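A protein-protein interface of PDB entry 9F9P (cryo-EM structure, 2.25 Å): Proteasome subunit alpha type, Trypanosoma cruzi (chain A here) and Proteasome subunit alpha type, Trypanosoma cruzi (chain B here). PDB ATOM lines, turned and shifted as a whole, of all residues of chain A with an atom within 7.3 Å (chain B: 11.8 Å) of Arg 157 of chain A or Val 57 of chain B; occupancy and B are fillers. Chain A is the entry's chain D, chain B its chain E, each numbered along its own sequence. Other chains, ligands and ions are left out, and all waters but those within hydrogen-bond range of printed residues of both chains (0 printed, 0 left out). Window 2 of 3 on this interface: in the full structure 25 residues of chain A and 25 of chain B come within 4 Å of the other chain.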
ATOM      1  N   GLY A  34     -22.543 -13.833  23.037  1.00  0.00           N
ATOM      2  CA  GLY A  34     -22.918 -12.474  23.407  1.00  0.00           C
ATOM      3  C   GLY A  34     -22.569 -11.463  22.310  1.00  0.00           C
ATOM      4  O   GLY A  34     -21.627 -11.677  21.556  1.00  0.00           O
ATOM      5  N   VAL A  35     -23.343 -10.376  22.228  1.00  0.00           N
ATOM      6  CA  VAL A  35     -23.218  -9.384  21.168  1.00  0.00           C
ATOM      7  C   VAL A  35     -23.524  -8.015  21.744  1.00  0.00           C
ATOM      8  O   VAL A  35     -24.551  -7.821  22.370  1.00  0.00           O
ATOM      9  CB  VAL A  35     -24.137  -9.676  19.964  1.00  0.00           C
ATOM     10  CG1 VAL A  35     -24.012  -8.590  18.922  1.00  0.00           C
ATOM     11  CG2 VAL A  35     -23.846 -11.030  19.319  1.00  0.00           C
ATOM     12  N   ARG A  36     -22.602  -7.083  21.548  1.00  0.00           N
ATOM     13  CA  ARG A  36     -22.744  -5.733  22.077  1.00  0.00           C
ATOM     14  C   ARG A  36     -23.199  -4.858  20.920  1.00  0.00           C
ATOM     15  O   ARG A  36     -22.562  -4.883  19.865  1.00  0.00           O
ATOM     16  CB  ARG A  36     -21.389  -5.288  22.632  1.00  0.00           C
ATOM     17  CG  ARG A  36     -21.430  -4.120  23.600  1.00  0.00           C
ATOM     18  CD  ARG A  36     -20.037  -3.615  23.948  1.00  0.00           C
ATOM     19  NE  ARG A  36     -19.494  -2.765  22.905  1.00  0.00           N
ATOM     20  CZ  ARG A  36     -18.200  -2.522  22.750  1.00  0.00           C
ATOM     21  NH1 ARG A  36     -17.328  -3.020  23.611  1.00  0.00           N
ATOM     22  NH2 ARG A  36     -17.776  -1.816  21.712  1.00  0.00           N
ATOM     23  N   GLY A  37     -24.317  -4.145  21.110  1.00  0.00           N
ATOM     24  CA  GLY A  37     -24.759  -3.144  20.148  1.00  0.00           C
ATOM     25  C   GLY A  37     -24.503  -1.717  20.632  1.00  0.00           C
ATOM     26  O   GLY A  37     -23.669  -1.503  21.504  1.00  0.00           O
ATOM     27  N   LEU A 144     -19.131  -5.889  27.844  1.00  0.00           N
ATOM     28  CA  LEU A 144     -19.241  -7.320  27.663  1.00  0.00           C
ATOM     29  C   LEU A 144     -17.883  -7.990  27.830  1.00  0.00           C
ATOM     30  O   LEU A 144     -16.966  -7.653  27.090  1.00  0.00           O
ATOM     31  CB  LEU A 144     -19.783  -7.554  26.265  1.00  0.00           C
ATOM     32  CG  LEU A 144     -19.885  -8.999  25.831  1.00  0.00           C
ATOM     33  CD1 LEU A 144     -21.042  -9.674  26.505  1.00  0.00           C
ATOM     34  CD2 LEU A 144     -20.086  -9.078  24.336  1.00  0.00           C
ATOM     35  N   ALA A 155     -12.248  -8.131  27.348  1.00  0.00           N
ATOM     36  CA  ALA A 155     -13.469  -7.490  26.870  1.00  0.00           C
ATOM     37  C   ALA A 155     -13.622  -7.710  25.382  1.00  0.00           C
ATOM     38  O   ALA A 155     -12.619  -7.740  24.675  1.00  0.00           O
ATOM     39  CB  ALA A 155     -13.430  -6.042  27.174  1.00  0.00           C
ATOM     40  N   TRP A 156     -14.867  -7.879  24.929  1.00  0.00           N
ATOM     41  CA  TRP A 156     -15.163  -8.237  23.549  1.00  0.00           C
ATOM     42  C   TRP A 156     -16.341  -7.414  23.035  1.00  0.00           C
ATOM     43  O   TRP A 156     -17.134  -6.875  23.806  1.00  0.00           O
ATOM     44  CB  TRP A 156     -15.520  -9.728  23.467  1.00  0.00           C
ATOM     45  CG  TRP A 156     -14.457 -10.695  23.874  1.00  0.00           C
ATOM     46  CD1 TRP A 156     -13.930 -10.885  25.118  1.00  0.00           C
ATOM     47  CD2 TRP A 156     -13.771 -11.612  23.016  1.00  0.00           C
ATOM     48  NE1 TRP A 156     -12.948 -11.840  25.085  1.00  0.00           N
ATOM     49  CE2 TRP A 156     -12.830 -12.308  23.814  1.00  0.00           C
ATOM     50  CE3 TRP A 156     -13.841 -11.897  21.648  1.00  0.00           C
ATOM     51  CZ2 TRP A 156     -11.976 -13.274  23.288  1.00  0.00           C
ATOM     52  CZ3 TRP A 156     -13.010 -12.864  21.130  1.00  0.00           C
ATOM     53  CH2 TRP A 156     -12.089 -13.542  21.941  1.00  0.00           C
ATOM     54  N   ARG A 157     -16.496  -7.359  21.712  1.00  0.00           N
ATOM     55  CA  ARG A 157     -17.654  -6.749  21.061  1.00  0.00           C
ATOM     56  C   ARG A 157     -18.701  -7.789  20.684  1.00  0.00           C
ATOM     57  O   ARG A 157     -19.891  -7.514  20.589  1.00  0.00           O
ATOM     58  CB  ARG A 157     -17.194  -6.101  19.752  1.00  0.00           C
ATOM     59  CG  ARG A 157     -16.335  -4.862  19.956  1.00  0.00           C
ATOM     60  CD  ARG A 157     -15.832  -4.382  18.611  1.00  0.00           C
ATOM     61  NE  ARG A 157     -14.520  -3.829  18.832  1.00  0.00           N
ATOM     62  CZ  ARG A 157     -13.418  -4.314  18.285  1.00  0.00           C
ATOM     63  NH1 ARG A 157     -13.508  -5.104  17.226  1.00  0.00           N
ATOM     64  NH2 ARG A 157     -12.238  -3.952  18.768  1.00  0.00           N
ATOM     65  N   ALA A 158     -18.200  -8.965  20.360  1.00  0.00           N
ATOM     66  CA  ALA A 158     -18.994 -10.157  20.247  1.00  0.00           C
ATOM     67  C   ALA A 158     -18.092 -11.333  20.582  1.00  0.00           C
ATOM     68  O   ALA A 158     -16.902 -11.270  20.307  1.00  0.00           O
ATOM     69  CB  ALA A 158     -19.523 -10.248  18.838  1.00  0.00           C
ATOM     70  N   VAL A 159     -18.672 -12.410  21.120  1.00  0.00           N
ATOM     71  CA  VAL A 159     -17.862 -13.534  21.558  1.00  0.00           C
ATOM     72  C   VAL A 159     -18.709 -14.790  21.668  1.00  0.00           C
ATOM     73  O   VAL A 159     -19.899 -14.667  21.902  1.00  0.00           O
ATOM     74  CB  VAL A 159     -17.195 -13.225  22.921  1.00  0.00           C
ATOM     75  CG1 VAL A 159     -18.197 -13.153  24.072  1.00  0.00           C
ATOM     76  CG2 VAL A 159     -16.106 -14.245  23.239  1.00  0.00           C
ATOM     77  N   MET A 172     -18.453 -14.727  13.049  1.00  0.00           N
ATOM     78  CA  MET A 172     -18.746 -13.436  13.664  1.00  0.00           C
ATOM     79  C   MET A 172     -17.669 -12.408  13.304  1.00  0.00           C
ATOM     80  O   MET A 172     -17.980 -11.226  13.216  1.00  0.00           O
ATOM     81  CB  MET A 172     -18.876 -13.555  15.192  1.00  0.00           C
ATOM     82  CG  MET A 172     -20.222 -14.128  15.636  1.00  0.00           C
ATOM     83  SD  MET A 172     -20.552 -14.277  17.443  1.00  0.00           S
ATOM     84  CE  MET A 172     -18.898 -14.123  18.107  1.00  0.00           C
ATOM     85  N   GLU A 173     -16.426 -12.865  13.080  1.00  0.00           N
ATOM     86  CA  GLU A 173     -15.304 -12.004  12.716  1.00  0.00           C
ATOM     87  C   GLU A 173     -15.564 -11.285  11.390  1.00  0.00           C
ATOM     88  O   GLU A 173     -15.196 -10.123  11.261  1.00  0.00           O
ATOM     89  CB  GLU A 173     -13.989 -12.798  12.640  1.00  0.00           C
ATOM     90  CG  GLU A 173     -13.245 -12.901  13.974  1.00  0.00           C
ATOM     91  CD  GLU A 173     -12.263 -14.056  14.150  1.00  0.00           C
ATOM     92  OE1 GLU A 173     -11.932 -14.721  13.143  1.00  0.00           O
ATOM     93  OE2 GLU A 173     -11.846 -14.308  15.307  1.00  0.00           O
ATOM     94  N   LYS A 174     -16.199 -11.975  10.423  1.00  0.00           N
ATOM     95  CA  LYS A 174     -16.485 -11.422   9.101  1.00  0.00           C
ATOM     96  C   LYS A 174     -17.607 -10.386   9.157  1.00  0.00           C
ATOM     97  O   LYS A 174     -17.423  -9.249   8.729  1.00  0.00           O
ATOM     98  CB  LYS A 174     -16.956 -12.494   8.109  1.00  0.00           C
ATOM     99  CG  LYS A 174     -16.054 -13.710   7.943  1.00  0.00           C
ATOM    100  CD  LYS A 174     -14.609 -13.397   7.607  1.00  0.00           C
ATOM    101  CE  LYS A 174     -13.893 -14.568   6.962  1.00  0.00           C
ATOM    102  NZ  LYS A 174     -14.102 -15.841   7.698  1.00  0.00           N
ATOM    103  N   TYR A 176     -19.591  -8.960  11.684  1.00  0.00           N
ATOM    104  CA  TYR A 176     -19.913  -8.005  12.742  1.00  0.00           C
ATOM    105  C   TYR A 176     -19.728  -6.582  12.214  1.00  0.00           C
ATOM    106  O   TYR A 176     -18.732  -6.303  11.544  1.00  0.00           O
ATOM    107  CB  TYR A 176     -19.055  -8.215  14.009  1.00  0.00           C
ATOM    108  CG  TYR A 176     -19.348  -7.266  15.158  1.00  0.00           C
ATOM    109  CD1 TYR A 176     -20.415  -7.483  16.013  1.00  0.00           C
ATOM    110  CD2 TYR A 176     -18.619  -6.098  15.350  1.00  0.00           C
ATOM    111  CE1 TYR A 176     -20.729  -6.600  17.041  1.00  0.00           C
ATOM    112  CE2 TYR A 176     -18.941  -5.180  16.346  1.00  0.00           C
ATOM    113  CZ  TYR A 176     -19.979  -5.452  17.223  1.00  0.00           C
ATOM    114  OH  TYR A 176     -20.302  -4.622  18.276  1.00  0.00           O
ATOM    115  N   GLN A 177     -20.685  -5.699  12.551  1.00  0.00           N
ATOM    116  CA  GLN A 177     -20.584  -4.271  12.268  1.00  0.00           C
ATOM    117  C   GLN A 177     -20.758  -3.493  13.569  1.00  0.00           C
ATOM    118  O   GLN A 177     -21.552  -3.892  14.418  1.00  0.00           O
ATOM    119  CB  GLN A 177     -21.678  -3.763  11.318  1.00  0.00           C
ATOM    120  CG  GLN A 177     -22.198  -4.777  10.301  1.00  0.00           C
ATOM    121  CD  GLN A 177     -23.563  -4.390   9.771  1.00  0.00           C
ATOM    122  OE1 GLN A 177     -24.524  -4.229  10.522  1.00  0.00           O
ATOM    123  NE2 GLN A 177     -23.660  -4.229   8.461  1.00  0.00           N
ATOM    124  N   GLU A 178     -20.068  -2.351  13.682  1.00  0.00           N
ATOM    125  CA  GLU A 178     -20.292  -1.414  14.774  1.00  0.00           C
ATOM    126  C   GLU A 178     -21.730  -0.877  14.766  1.00  0.00           C
ATOM    127  O   GLU A 178     -22.395  -0.845  13.734  1.00  0.00           O
ATOM    128  CB  GLU A 178     -19.298  -0.249  14.690  1.00  0.00           C
ATOM    129  CG  GLU A 178     -18.172  -0.304  15.717  1.00  0.00           C
ATOM    130  CD  GLU A 178     -17.225  -1.490  15.618  1.00  0.00           C
ATOM    131  OE1 GLU A 178     -16.725  -1.759  14.505  1.00  0.00           O
ATOM    132  OE2 GLU A 178     -16.972  -2.131  16.659  1.00  0.00           O
ATOM    133  N   MET A 180     -25.089  -1.418  16.034  1.00  0.00           N
ATOM    134  CA  MET A 180     -26.237  -2.139  15.516  1.00  0.00           C
ATOM    135  C   MET A 180     -27.446  -1.847  16.402  1.00  0.00           C
ATOM    136  O   MET A 180     -27.313  -1.449  17.560  1.00  0.00           O
ATOM    137  CB  MET A 180     -25.977  -3.650  15.491  1.00  0.00           C
ATOM    138  CG  MET A 180     -25.239  -4.126  14.250  1.00  0.00           C
ATOM    139  SD  MET A 180     -25.240  -5.938  14.030  1.00  0.00           S
ATOM    140  CE  MET A 180     -24.445  -6.497  15.535  1.00  0.00           C
ATOM    141  N   PHE A 188     -28.382 -11.051  14.353  1.00  0.00           N
ATOM    142  CA  PHE A 188     -26.987 -11.453  14.239  1.00  0.00           C
ATOM    143  C   PHE A 188     -26.637 -12.610  15.188  1.00  0.00           C
ATOM    144  O   PHE A 188     -25.875 -13.505  14.826  1.00  0.00           O
ATOM    145  CB  PHE A 188     -26.105 -10.243  14.527  1.00  0.00           C
ATOM    146  CG  PHE A 188     -24.629 -10.503  14.404  1.00  0.00           C
ATOM    147  CD1 PHE A 188     -23.857 -10.753  15.531  1.00  0.00           C
ATOM    148  CD2 PHE A 188     -24.005 -10.455  13.174  1.00  0.00           C
ATOM    149  CE1 PHE A 188     -22.490 -10.977  15.422  1.00  0.00           C
ATOM    150  CE2 PHE A 188     -22.638 -10.675  13.067  1.00  0.00           C
ATOM    151  CZ  PHE A 188     -21.882 -10.940  14.189  1.00  0.00           C
ATOM    152  N   LYS B  52       1.694  -7.143  22.611  1.00  0.00           N
ATOM    153  CA  LYS B  52       0.359  -7.376  23.150  1.00  0.00           C
ATOM    154  C   LYS B  52      -0.179  -8.782  22.849  1.00  0.00           C
ATOM    155  O   LYS B  52      -0.467  -9.534  23.782  1.00  0.00           O
ATOM    156  CB  LYS B  52      -0.647  -6.357  22.630  1.00  0.00           C
ATOM    157  CG  LYS B  52      -0.847  -5.152  23.530  1.00  0.00           C
ATOM    158  CD  LYS B  52      -1.974  -4.274  23.062  1.00  0.00           C
ATOM    159  CE  LYS B  52      -2.615  -3.486  24.181  1.00  0.00           C
ATOM    160  NZ  LYS B  52      -3.552  -2.472  23.634  1.00  0.00           N
ATOM    161  N   ARG B  53      -0.382  -9.116  21.568  1.00  0.00           N
ATOM    162  CA  ARG B  53      -0.838 -10.443  21.156  1.00  0.00           C
ATOM    163  C   ARG B  53      -2.294 -10.695  21.569  1.00  0.00           C
ATOM    164  O   ARG B  53      -2.547 -11.412  22.530  1.00  0.00           O
ATOM    165  CB  ARG B  53       0.073 -11.546  21.720  1.00  0.00           C
ATOM    166  CG  ARG B  53      -0.176 -12.932  21.135  1.00  0.00           C
ATOM    167  CD  ARG B  53       0.509 -14.059  21.899  1.00  0.00           C
ATOM    168  NE  ARG B  53       1.901 -14.278  21.520  1.00  0.00           N
ATOM    169  CZ  ARG B  53       2.702 -15.195  22.064  1.00  0.00           C
ATOM    170  NH1 ARG B  53       3.957 -15.303  21.665  1.00  0.00           N
ATOM    171  NH2 ARG B  53       2.252 -15.997  23.018  1.00  0.00           N
ATOM    172  N   VAL B  54      -3.248 -10.151  20.794  1.00  0.00           N
ATOM    173  CA  VAL B  54      -4.666 -10.382  21.022  1.00  0.00           C
ATOM    174  C   VAL B  54      -5.127 -11.575  20.186  1.00  0.00           C
ATOM    175  O   VAL B  54      -4.671 -11.750  19.058  1.00  0.00           O
ATOM    176  CB  VAL B  54      -5.531  -9.144  20.705  1.00  0.00           C
ATOM    177  CG1 VAL B  54      -5.047  -7.898  21.429  1.00  0.00           C
ATOM    178  CG2 VAL B  54      -5.635  -8.889  19.211  1.00  0.00           C
ATOM    179  N   PRO B  55      -6.084 -12.388  20.704  1.00  0.00           N
ATOM    180  CA  PRO B  55      -6.617 -13.548  19.975  1.00  0.00           C
ATOM    181  C   PRO B  55      -7.562 -13.303  18.784  1.00  0.00           C
ATOM    182  O   PRO B  55      -7.667 -14.167  17.915  1.00  0.00           O
ATOM    183  CB  PRO B  55      -7.365 -14.363  21.051  1.00  0.00           C
ATOM    184  CG  PRO B  55      -7.636 -13.402  22.203  1.00  0.00           C
ATOM    185  CD  PRO B  55      -6.663 -12.250  22.051  1.00  0.00           C
ATOM    186  N   SER B  56      -8.260 -12.156  18.724  1.00  0.00           N
ATOM    187  CA  SER B  56      -9.073 -11.847  17.554  1.00  0.00           C
ATOM    188  C   SER B  56      -9.352 -10.347  17.430  1.00  0.00           C
ATOM    189  O   SER B  56      -9.153  -9.586  18.376  1.00  0.00           O
ATOM    190  CB  SER B  56     -10.361 -12.642  17.561  1.00  0.00           C
ATOM    191  OG  SER B  56     -11.270 -12.144  18.520  1.00  0.00           O
ATOM    192  N   VAL B  57      -9.864  -9.936  16.263  1.00  0.00           N
ATOM    193  CA  VAL B  57     -10.178  -8.534  16.025  1.00  0.00           C
ATOM    194  C   VAL B  57     -11.380  -8.085  16.864  1.00  0.00           C
ATOM    195  O   VAL B  57     -11.605  -6.885  17.006  1.00  0.00           O
ATOM    196  CB  VAL B  57     -10.407  -8.224  14.528  1.00  0.00           C
ATOM    197  CG1 VAL B  57      -9.200  -8.616  13.685  1.00  0.00           C
ATOM    198  CG2 VAL B  57     -11.678  -8.865  13.971  1.00  0.00           C
ATOM    199  N   LEU B  58     -12.143  -9.029  17.437  1.00  0.00           N
ATOM    200  CA  LEU B  58     -13.333  -8.689  18.208  1.00  0.00           C
ATOM    201  C   LEU B  58     -13.020  -8.258  19.640  1.00  0.00           C
ATOM    202  O   LEU B  58     -13.916  -7.803  20.332  1.00  0.00           O
ATOM    203  CB  LEU B  58     -14.260  -9.898  18.210  1.00  0.00           C
ATOM    204  CG  LEU B  58     -14.794 -10.303  16.837  1.00  0.00           C
ATOM    205  CD1 LEU B  58     -15.513 -11.649  16.906  1.00  0.00           C
ATOM    206  CD2 LEU B  58     -15.714  -9.222  16.306  1.00  0.00           C
ATOM    207  N   VAL B  59     -11.759  -8.366  20.056  1.00  0.00           N
ATOM    208  CA  VAL B  59     -11.321  -7.998  21.391  1.00  0.00           C
ATOM    209  C   VAL B  59     -10.949  -6.520  21.438  1.00  0.00           C
ATOM    210  O   VAL B  59     -10.192  -6.063  20.588  1.00  0.00           O
ATOM    211  CB  VAL B  59     -10.123  -8.863  21.807  1.00  0.00           C
ATOM    212  CG1 VAL B  59      -9.500  -8.374  23.097  1.00  0.00           C
ATOM    213  CG2 VAL B  59     -10.502 -10.323  21.950  1.00  0.00           C
ATOM    214  N   ASP B  60     -11.464  -5.798  22.445  1.00  0.00           N
ATOM    215  CA  ASP B  60     -10.996  -4.457  22.777  1.00  0.00           C
ATOM    216  C   ASP B  60      -9.568  -4.501  23.323  1.00  0.00           C
ATOM    217  O   ASP B  60      -9.352  -5.002  24.427  1.00  0.00           O
ATOM    218  CB  ASP B  60     -11.861  -3.782  23.847  1.00  0.00           C
ATOM    219  CG  ASP B  60     -13.272  -3.479  23.386  1.00  0.00           C
ATOM    220  OD1 ASP B  60     -13.744  -4.190  22.475  1.00  0.00           O
ATOM    221  OD2 ASP B  60     -13.870  -2.512  23.918  1.00  0.00           O
ATOM    222  N   PRO B  61      -8.549  -3.958  22.610  1.00  0.00           N
ATOM    223  CA  PRO B  61      -7.161  -4.106  23.056  1.00  0.00           C
ATOM    224  C   PRO B  61      -6.857  -3.401  24.386  1.00  0.00           C
ATOM    225  O   PRO B  61      -5.953  -3.821  25.111  1.00  0.00           O
ATOM    226  CB  PRO B  61      -6.354  -3.574  21.854  1.00  0.00           C
ATOM    227  CG  PRO B  61      -7.324  -3.610  20.694  1.00  0.00           C
ATOM    228  CD  PRO B  61      -8.650  -3.235  21.326  1.00  0.00           C
ATOM    229  N   SER B  62      -7.651  -2.376  24.737  1.00  0.00           N
ATOM    230  CA  SER B  62      -7.552  -1.692  26.026  1.00  0.00           C
ATOM    231  C   SER B  62      -7.512  -2.675  27.204  1.00  0.00           C
ATOM    232  O   SER B  62      -6.745  -2.492  28.146  1.00  0.00           O
ATOM    233  CB  SER B  62      -8.705  -0.717  26.195  1.00  0.00           C
ATOM    234  OG  SER B  62      -8.954  -0.017  24.981  1.00  0.00           O
ATOM    235  N   SER B  63      -8.344  -3.727  27.127  1.00  0.00           N
ATOM    236  CA  SER B  63      -8.626  -4.635  28.230  1.00  0.00           C
ATOM    237  C   SER B  63      -7.498  -5.636  28.485  1.00  0.00           C
ATOM    238  O   SER B  63      -7.596  -6.445  29.406  1.00  0.00           O
ATOM    239  CB  SER B  63      -9.913  -5.376  27.961  1.00  0.00           C
ATOM    240  OG  SER B  63      -9.744  -6.454  27.043  1.00  0.00           O
ATOM    241  N   MET B  64      -6.443  -5.606  27.664  1.00  0.00           N
ATOM    242  CA  MET B  64      -5.412  -6.629  27.719  1.00  0.00           C
ATOM    243  C   MET B  64      -4.049  -6.014  28.039  1.00  0.00           C
ATOM    244  O   MET B  64      -3.043  -6.475  27.507  1.00  0.00           O
ATOM    245  CB  MET B  64      -5.336  -7.357  26.374  1.00  0.00           C
ATOM    246  CG  MET B  64      -6.427  -8.403  26.190  1.00  0.00           C
ATOM    247  SD  MET B  64      -5.913  -9.743  25.085  1.00  0.00           S
ATOM    248  CE  MET B  64      -6.200 -11.191  26.104  1.00  0.00           C
ATOM    249  N   GLU B 208       3.355 -11.482  13.886  1.00  0.00           N
ATOM    250  CA  GLU B 208       2.509 -10.647  13.043  1.00  0.00           C
ATOM    251  C   GLU B 208       3.313  -9.468  12.498  1.00  0.00           C
ATOM    252  O   GLU B 208       4.518  -9.375  12.717  1.00  0.00           O
ATOM    253  CB  GLU B 208       1.319 -10.102  13.843  1.00  0.00           C
ATOM    254  CG  GLU B 208       0.346 -11.155  14.343  1.00  0.00           C
ATOM    255  CD  GLU B 208      -0.551 -10.673  15.474  1.00  0.00           C
ATOM    256  OE1 GLU B 208      -0.042 -10.515  16.609  1.00  0.00           O
ATOM    257  OE2 GLU B 208      -1.750 -10.435  15.218  1.00  0.00           O
ATOM    258  N   GLU B 209       2.617  -8.569  11.789  1.00  0.00           N
ATOM    259  CA  GLU B 209       3.178  -7.303  11.346  1.00  0.00           C
ATOM    260  C   GLU B 209       2.859  -6.222  12.375  1.00  0.00           C
ATOM    261  O   GLU B 209       1.738  -6.136  12.872  1.00  0.00           O
ATOM    262  CB  GLU B 209       2.620  -6.922   9.973  1.00  0.00           C
ATOM    263  CG  GLU B 209       2.894  -7.961   8.898  1.00  0.00           C
ATOM    264  CD  GLU B 209       2.276  -7.669   7.539  1.00  0.00           C
ATOM    265  OE1 GLU B 209       1.719  -6.566   7.363  1.00  0.00           O
ATOM    266  OE2 GLU B 209       2.345  -8.552   6.659  1.00  0.00           O
ATOM    267  N   THR B 211       1.950  -3.086  14.128  1.00  0.00           N
ATOM    268  CA  THR B 211       1.170  -1.863  14.061  1.00  0.00           C
ATOM    269  C   THR B 211       1.389  -1.072  15.348  1.00  0.00           C
ATOM    270  O   THR B 211       2.195  -1.463  16.186  1.00  0.00           O
ATOM    271  CB  THR B 211      -0.319  -2.160  13.816  1.00  0.00           C
ATOM    272  OG1 THR B 211      -0.899  -2.667  15.021  1.00  0.00           O
ATOM    273  CG2 THR B 211      -0.550  -3.138  12.681  1.00  0.00           C
ATOM    274  N   SER B 213      -1.115  -0.487  17.481  1.00  0.00           N
ATOM    275  CA  SER B 213      -2.150  -0.882  18.431  1.00  0.00           C
ATOM    276  C   SER B 213      -1.948  -2.339  18.843  1.00  0.00           C
ATOM    277  O   SER B 213      -2.885  -3.018  19.257  1.00  0.00           O
ATOM    278  CB  SER B 213      -3.537  -0.644  17.864  1.00  0.00           C
ATOM    279  OG  SER B 213      -3.863  -1.591  16.853  1.00  0.00           O
ATOM    280  N   ASN B 214      -0.692  -2.779  18.748  1.00  0.00           N
ATOM    281  CA  ASN B 214      -0.310  -4.172  18.881  1.00  0.00           C
ATOM    282  C   ASN B 214       0.906  -4.280  19.812  1.00  0.00           C
ATOM    283  O   ASN B 214       1.435  -5.374  20.015  1.00  0.00           O
ATOM    284  CB  ASN B 214      -0.055  -4.724  17.474  1.00  0.00           C
ATOM    285  CG  ASN B 214       0.398  -6.163  17.436  1.00  0.00           C
ATOM    286  OD1 ASN B 214       0.036  -6.959  18.301  1.00  0.00           O
ATOM    287  ND2 ASN B 214       1.184  -6.504  16.427  1.00  0.00           N
ATOM    288  N   GLN B 232      -1.235   5.783  21.207  1.00  0.00           N
ATOM    289  CA  GLN B 232      -1.048   5.200  19.882  1.00  0.00           C
ATOM    290  C   GLN B 232      -0.328   6.198  18.971  1.00  0.00           C
ATOM    291  O   GLN B 232       0.611   5.833  18.260  1.00  0.00           O
ATOM    292  CB  GLN B 232      -2.402   4.780  19.305  1.00  0.00           C
ATOM    293  CG  GLN B 232      -3.131   3.743  20.148  1.00  0.00           C
ATOM    294  CD  GLN B 232      -4.456   3.349  19.543  1.00  0.00           C
ATOM    295  OE1 GLN B 232      -5.361   4.169  19.392  1.00  0.00           O
ATOM    296  NE2 GLN B 232      -4.580   2.081  19.186  1.00  0.00           N
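The guanidinium group (NH1) of Arg 36 of chain A is in salt-bridge range of the side-chain carboxylate (OD2) of Asp 60 of chain B (3.5 Å).
The backbone NH of Asp 60 of chain B lies within hydrogen-bond range of the backbone carbonyl oxygen of Ala 155 of chain A, at 3.2 Å.
OG of Ser 63 of chain B lies within hydrogen-bond range of N of Ala 155 of chain A (3.0 Å).
The backbone carbonyl oxygen of Val 57 of chain B is in hydrogen-bond range of the guanidinium group of Arg 157 of chain A, at 2.6 Å.
The backbone NH (N) of Arg 157 of chain A is in hydrogen-bond range of the backbone carbonyl oxygen (O) of Leu 58 of chain B, 3.0 Å away.
The backbone carbonyl oxygen (O) of Val 59 of chain B sits at hydrogen-bond distance from the guanidinium group (NH2) of Arg 157 of chain A (3.5 Å).
The guanidinium group of Arg 157 of chain A is in salt-bridge range of the side-chain carboxylate of Asp 60 of chain B.
N of Arg 36 of chain A lies within hydrogen-bond range of O of Arg 157 of chain A, 2.9 Å away.
OH of Tyr 176 of chain A lies within hydrogen-bond range of O of Arg 36 of chain A (2.8 Å).
The backbone carbonyl oxygen of Leu 144 of chain A is in hydrogen-bond range of the backbone NH of Trp 156 of chain A.
The guanidinium group (NE) of Arg 157 of chain A lies within salt-bridge range of the side-chain carboxylate (OE2) of Glu 178 of chain A.
The side-chain hydroxyl of Ser 56 of chain B sits close to the backbone NH of Leu 58 of chain B (3.4 Å).
O of Asp 60 of chain B lies within hydrogen-bond range of OG of Ser 63 of chain B, 3.0 Å away.
Ala 155 of chain A touches Val 59 of chain B.
Ser 56 of chain B touches Trp 156 of chain A.
Trp 156 of chain A touches Leu 58 of chain B (CA to O, 3.5 Å).
CZ2 of Trp 156 of chain A touches CG2 of Val 59 of chain B (3.6 Å).
Ala 158 of chain A touches Leu 58 of chain B.
CB of Ser 56 of chain B touches OE2 of Glu 173 of chain A (3.2 Å).
Glu 173 of chain A touches Leu 58 of chain B.
Of chain B, only Val 57, Leu 58, Val 59 and Asp 60 come within 4 Å of Arg 157 of chain A.
Of chain A, only Arg 157 (2.6 Å) comes within 4 Å of Val 57 of chain B.
No residue of chain B comes within 4 Å of Leu 144 of chain A.
Ala 155 of chain A touches just these residues of chain B: Val 59 (3.5 Å), Asp 60 (3.2 Å) and Ser 63 (3.0 Å).
Ala 158 of chain A touches just one residue of chain B: Leu 58.
No residue of chain B comes within 4 Å of Val 159 of chain A.
Glu 173 of chain A touches just these residues of chain B: Ser 56 (3.2 Å) and Leu 58 (3.9 Å).
Of the printed residues of chain A, Asp 60 of chain B touches Arg 36, Ala 155 and Arg 157.
Of the printed residues of chain A, Ser 56 of chain B touches Trp 156 and Glu 173.
Of the printed residues of chain A, Leu 58 of chain B touches Trp 156 (3.5 Å), Arg 157 (3.0 Å), Ala 158 (3.6 Å) and Glu 173 (3.9 Å).
Printed residues of chain A within 4 Å of Ser 63 of chain B: Ala 155 (3.0 Å).
Of the printed residues of chain A, Val 59 of chain B touches Ala 155, Trp 156 and Arg 157.
Met 64 of chain B touches none of the printed residues of chain A.
The nearest residue of chain B that does not touch Arg 157 of chain A is Pro 61 of chain B (4.5 Å).
The nearest residue of chain A that does not touch Val 57 of chain B is Glu 173 of chain A (4.3 Å).
The nearest printed residue of chain A that does not touch Leu 58 of chain B is Tyr 176 of chain A (4.2 Å).
Printed residues of chain A that touch a printed residue of chain B: Arg 36, Ala 155, Trp 156, Arg 157, Ala 158 and Glu 173.
Hydrophobic or aromatic side chains of chain A within 4 Å of the printed part of chain B: Ala 155 and Trp 156.
Hydrophobic or aromatic side chains of chain B within 4 Å of the printed part of chain A: Leu 58 and Val 59.
Along chain B the printed residues that touch a printed residue of chain A span positions 56 to 63.
Among the printed residues, 14 pairs touch across the chains.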
